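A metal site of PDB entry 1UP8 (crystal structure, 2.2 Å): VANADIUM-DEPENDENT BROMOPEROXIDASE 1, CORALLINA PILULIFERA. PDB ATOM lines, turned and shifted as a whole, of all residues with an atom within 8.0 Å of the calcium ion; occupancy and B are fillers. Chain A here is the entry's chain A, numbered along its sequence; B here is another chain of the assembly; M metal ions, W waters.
The calcium ion is bound by water W1 (2.3 Å).
The calcium ion is bound by O of Gln 370, 2.4 Å away.
The calcium ion is bound by O of Gln 363 (2.4 Å).
OD1 of Asp 365 is bound to the calcium ion (2.4 Å).
The calcium ion is bound by O of Phe 361 (2.5 Å).
OD2 of Asp 368 binds the calcium ion (2.6 Å).
The calcium ion is bound by OD1 of Asp 368 (2.6 Å).
Of the 16 residues printed, 5 come within 4 Å of the calcium ion.
The backbone carbonyl oxygen (O) of Asp 365 sits close to the side-chain amide oxygen (OD1) of Asn 369 (3.5 Å).
O of Trp 125 of chain B lies close to NE2 of Gln 370, at 3.4 Å.
The side-chain carboxylate (OD2) of Asp 365 is in hydrogen-bond range of the backbone NH (N) of Gly 124 of chain B, at 2.8 Å.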
ATOM      1  N   PRO A 360      27.643  -9.430   9.711  1.00  0.00           N
ATOM      2  CA  PRO A 360      27.266 -10.671  10.411  1.00  0.00           C
ATOM      3  C   PRO A 360      27.788 -10.714  11.838  1.00  0.00           C
ATOM      4  O   PRO A 360      28.747 -10.013  12.162  1.00  0.00           O
ATOM      5  CB  PRO A 360      27.917 -11.788   9.569  1.00  0.00           C
ATOM      6  CG  PRO A 360      28.736 -11.119   8.504  1.00  0.00           C
ATOM      7  CD  PRO A 360      28.789  -9.638   8.810  1.00  0.00           C
ATOM      8  N   PHE A 361      27.119 -11.512  12.667  1.00  0.00           N
ATOM      9  CA  PHE A 361      27.658 -11.968  13.947  1.00  0.00           C
ATOM     10  C   PHE A 361      27.635 -10.862  14.995  1.00  0.00           C
ATOM     11  O   PHE A 361      28.275 -10.974  16.060  1.00  0.00           O
ATOM     12  CB  PHE A 361      29.065 -12.604  13.791  1.00  0.00           C
ATOM     13  CG  PHE A 361      29.154 -13.717  12.747  1.00  0.00           C
ATOM     14  CD1 PHE A 361      30.275 -13.836  11.926  1.00  0.00           C
ATOM     15  CD2 PHE A 361      28.130 -14.680  12.625  1.00  0.00           C
ATOM     16  CE1 PHE A 361      30.384 -14.888  10.973  1.00  0.00           C
ATOM     17  CE2 PHE A 361      28.224 -15.741  11.674  1.00  0.00           C
ATOM     18  CZ  PHE A 361      29.348 -15.837  10.836  1.00  0.00           C
ATOM     19  N   GLN A 362      26.879  -9.790  14.736  1.00  0.00           N
ATOM     20  CA  GLN A 362      26.873  -8.665  15.679  1.00  0.00           C
ATOM     21  C   GLN A 362      25.928  -8.839  16.887  1.00  0.00           C
ATOM     22  O   GLN A 362      25.871  -7.970  17.760  1.00  0.00           O
ATOM     23  CB  GLN A 362      26.631  -7.319  14.958  1.00  0.00           C
ATOM     24  CG  GLN A 362      27.599  -6.996  13.810  1.00  0.00           C
ATOM     25  CD  GLN A 362      29.069  -6.983  14.249  1.00  0.00           C
ATOM     26  OE1 GLN A 362      29.413  -6.511  15.357  1.00  0.00           O
ATOM     27  NE2 GLN A 362      29.935  -7.489  13.382  1.00  0.00           N
ATOM     28  N   GLN A 363      25.202  -9.970  16.939  1.00  0.00           N
ATOM     29  CA  GLN A 363      24.247 -10.208  18.014  1.00  0.00           C
ATOM     30  C   GLN A 363      24.950 -10.801  19.241  1.00  0.00           C
ATOM     31  O   GLN A 363      26.120 -11.266  19.158  1.00  0.00           O
ATOM     32  CB  GLN A 363      23.175 -11.179  17.558  1.00  0.00           C
ATOM     33  CG  GLN A 363      22.165 -10.618  16.578  1.00  0.00           C
ATOM     34  CD  GLN A 363      21.303 -11.732  16.025  1.00  0.00           C
ATOM     35  OE1 GLN A 363      21.686 -12.444  15.087  1.00  0.00           O
ATOM     36  NE2 GLN A 363      20.139 -11.910  16.622  1.00  0.00           N
ATOM     37  N   GLU A 364      24.252 -10.759  20.381  1.00  0.00           N
ATOM     38  CA  GLU A 364      24.671 -11.469  21.610  1.00  0.00           C
ATOM     39  C   GLU A 364      25.032 -12.939  21.257  1.00  0.00           C
ATOM     40  O   GLU A 364      24.317 -13.605  20.509  1.00  0.00           O
ATOM     41  CB  GLU A 364      23.501 -11.486  22.614  1.00  0.00           C
ATOM     42  CG  GLU A 364      23.542 -10.595  23.820  1.00  0.00           C
ATOM     43  CD  GLU A 364      22.557 -11.106  24.845  1.00  0.00           C
ATOM     44  OE1 GLU A 364      21.358 -11.185  24.499  1.00  0.00           O
ATOM     45  OE2 GLU A 364      22.976 -11.502  25.947  1.00  0.00           O
ATOM     46  N   ASP A 365      26.118 -13.437  21.812  1.00  0.00           N
ATOM     47  CA  ASP A 365      26.679 -14.705  21.386  1.00  0.00           C
ATOM     48  C   ASP A 365      25.787 -15.913  21.727  1.00  0.00           C
ATOM     49  O   ASP A 365      25.889 -16.943  21.066  1.00  0.00           O
ATOM     50  CB  ASP A 365      28.121 -14.877  21.931  1.00  0.00           C
ATOM     51  CG  ASP A 365      29.157 -14.027  21.175  1.00  0.00           C
ATOM     52  OD1 ASP A 365      28.774 -13.252  20.259  1.00  0.00           O
ATOM     53  OD2 ASP A 365      30.399 -14.078  21.433  1.00  0.00           O
ATOM     54  N   LYS A 366      24.892 -15.791  22.728  1.00  0.00           N
ATOM     55  CA  LYS A 366      23.948 -16.881  23.021  1.00  0.00           C
ATOM     56  C   LYS A 366      23.016 -17.082  21.818  1.00  0.00           C
ATOM     57  O   LYS A 366      22.500 -18.202  21.622  1.00  0.00           O
ATOM     58  CB  LYS A 366      23.121 -16.631  24.305  1.00  0.00           C
ATOM     59  CG  LYS A 366      22.089 -15.468  24.178  1.00  0.00           C
ATOM     60  CD  LYS A 366      20.939 -15.539  25.187  1.00  0.00           C
ATOM     61  CE  LYS A 366      20.491 -14.125  25.550  1.00  0.00           C
ATOM     62  NZ  LYS A 366      19.119 -14.064  26.130  1.00  0.00           N
ATOM     63  N   LEU A 367      22.830 -16.012  21.017  1.00  0.00           N
ATOM     64  CA  LEU A 367      21.963 -16.065  19.816  1.00  0.00           C
ATOM     65  C   LEU A 367      22.687 -16.596  18.545  1.00  0.00           C
ATOM     66  O   LEU A 367      22.189 -17.510  17.898  1.00  0.00           O
ATOM     67  CB  LEU A 367      21.283 -14.708  19.529  1.00  0.00           C
ATOM     68  CG  LEU A 367      20.307 -14.141  20.597  1.00  0.00           C
ATOM     69  CD1 LEU A 367      19.762 -12.781  20.238  1.00  0.00           C
ATOM     70  CD2 LEU A 367      19.138 -15.110  20.858  1.00  0.00           C
ATOM     71  N   ASP A 368      23.880 -16.052  18.245  1.00  0.00           N
ATOM     72  CA  ASP A 368      24.634 -16.412  17.030  1.00  0.00           C
ATOM     73  C   ASP A 368      25.856 -17.336  17.200  1.00  0.00           C
ATOM     74  O   ASP A 368      26.455 -17.738  16.203  1.00  0.00           O
ATOM     75  CB  ASP A 368      25.014 -15.161  16.181  1.00  0.00           C
ATOM     76  CG  ASP A 368      25.929 -14.194  16.918  1.00  0.00           C
ATOM     77  OD1 ASP A 368      26.615 -14.574  17.922  1.00  0.00           O
ATOM     78  OD2 ASP A 368      26.037 -12.999  16.557  1.00  0.00           O
ATOM     79  N   ASN A 369      26.238 -17.683  18.428  1.00  0.00           N
ATOM     80  CA  ASN A 369      27.415 -18.539  18.641  1.00  0.00           C
ATOM     81  C   ASN A 369      28.715 -18.007  17.957  1.00  0.00           C
ATOM     82  O   ASN A 369      29.609 -18.805  17.636  1.00  0.00           O
ATOM     83  CB  ASN A 369      27.130 -19.985  18.179  1.00  0.00           C
ATOM     84  CG  ASN A 369      26.027 -20.671  19.015  1.00  0.00           C
ATOM     85  OD1 ASN A 369      25.753 -20.280  20.156  1.00  0.00           O
ATOM     86  ND2 ASN A 369      25.386 -21.707  18.429  1.00  0.00           N
ATOM     87  N   GLN A 370      28.821 -16.681  17.754  1.00  0.00           N
ATOM     88  CA  GLN A 370      29.973 -16.132  17.009  1.00  0.00           C
ATOM     89  C   GLN A 370      30.425 -14.716  17.389  1.00  0.00           C
ATOM     90  O   GLN A 370      29.669 -13.747  17.278  1.00  0.00           O
ATOM     91  CB  GLN A 370      29.746 -16.233  15.499  1.00  0.00           C
ATOM     92  CG  GLN A 370      31.015 -16.077  14.622  1.00  0.00           C
ATOM     93  CD  GLN A 370      31.791 -17.391  14.315  1.00  0.00           C
ATOM     94  OE1 GLN A 370      32.757 -17.365  13.555  1.00  0.00           O
ATOM     95  NE2 GLN A 370      31.383 -18.504  14.911  1.00  0.00           N
ATOM     96  N   ASP A 371      31.677 -14.593  17.844  1.00  0.00           N
ATOM     97  CA  ASP A 371      32.285 -13.291  18.111  1.00  0.00           C
ATOM     98  C   ASP A 371      33.101 -12.896  16.885  1.00  0.00           C
ATOM     99  O   ASP A 371      33.321 -13.733  15.983  1.00  0.00           O
ATOM    100  CB  ASP A 371      33.146 -13.346  19.385  1.00  0.00           C
ATOM    101  CG  ASP A 371      33.369 -11.974  20.033  1.00  0.00           C
ATOM    102  OD1 ASP A 371      32.939 -10.926  19.495  1.00  0.00           O
ATOM    103  OD2 ASP A 371      34.043 -11.850  21.084  1.00  0.00           O
ATOM    104  N   VAL A 372      33.543 -11.642  16.824  1.00  0.00           N
ATOM    105  CA  VAL A 372      34.191 -11.083  15.629  1.00  0.00           C
ATOM    106  C   VAL A 372      35.577 -10.503  15.894  1.00  0.00           C
ATOM    107  O   VAL A 372      35.788  -9.878  16.923  1.00  0.00           O
ATOM    108  CB  VAL A 372      33.303  -9.996  14.966  1.00  0.00           C
ATOM    109  CG1 VAL A 372      32.001 -10.649  14.376  1.00  0.00           C
ATOM    110  CG2 VAL A 372      33.004  -8.837  15.987  1.00  0.00           C
ATOM    111  N   ARG B 123      30.368 -16.656  25.882  1.00  0.00           N
ATOM    112  CA  ARG B 123      30.989 -15.996  24.711  1.00  0.00           C
ATOM    113  C   ARG B 123      31.189 -17.034  23.602  1.00  0.00           C
ATOM    114  O   ARG B 123      31.312 -18.238  23.900  1.00  0.00           O
ATOM    115  CB  ARG B 123      32.365 -15.393  25.066  1.00  0.00           C
ATOM    116  CG  ARG B 123      33.348 -16.409  25.691  1.00  0.00           C
ATOM    117  CD  ARG B 123      34.727 -15.892  25.965  1.00  0.00           C
ATOM    118  NE  ARG B 123      35.386 -15.305  24.781  1.00  0.00           N
ATOM    119  CZ  ARG B 123      36.700 -15.096  24.700  1.00  0.00           C
ATOM    120  NH1 ARG B 123      37.473 -15.458  25.723  1.00  0.00           N
ATOM    121  NH2 ARG B 123      37.241 -14.520  23.620  1.00  0.00           N
ATOM    122  N   GLY B 124      31.274 -16.583  22.350  1.00  0.00           N
ATOM    123  CA  GLY B 124      31.365 -17.501  21.208  1.00  0.00           C
ATOM    124  C   GLY B 124      32.663 -17.517  20.403  1.00  0.00           C
ATOM    125  O   GLY B 124      33.581 -16.711  20.590  1.00  0.00           O
ATOM    126  N   TRP B 125      32.737 -18.467  19.468  1.00  0.00           N
ATOM    127  CA  TRP B 125      33.925 -18.631  18.634  1.00  0.00           C
ATOM    128  C   TRP B 125      34.189 -17.400  17.737  1.00  0.00           C
ATOM    129  O   TRP B 125      33.249 -16.784  17.194  1.00  0.00           O
ATOM    130  CB  TRP B 125      33.830 -19.930  17.827  1.00  0.00           C
ATOM    131  CG  TRP B 125      33.652 -21.152  18.741  1.00  0.00           C
ATOM    132  CD1 TRP B 125      34.621 -21.728  19.518  1.00  0.00           C
ATOM    133  CD2 TRP B 125      32.440 -21.891  19.000  1.00  0.00           C
ATOM    134  NE1 TRP B 125      34.093 -22.772  20.229  1.00  0.00           N
ATOM    135  CE2 TRP B 125      32.765 -22.908  19.926  1.00  0.00           C
ATOM    136  CE3 TRP B 125      31.111 -21.808  18.531  1.00  0.00           C
ATOM    137  CZ2 TRP B 125      31.814 -23.849  20.391  1.00  0.00           C
ATOM    138  CZ3 TRP B 125      30.144 -22.745  18.987  1.00  0.00           C
ATOM    139  CH2 TRP B 125      30.510 -23.754  19.904  1.00  0.00           C
HETATM  140 CA    CA M   1      27.999 -12.335  18.160  1.00  0.00          CA
HETATM  141  O   HOH W   1      29.338 -10.547  18.805  1.00  0.00           O
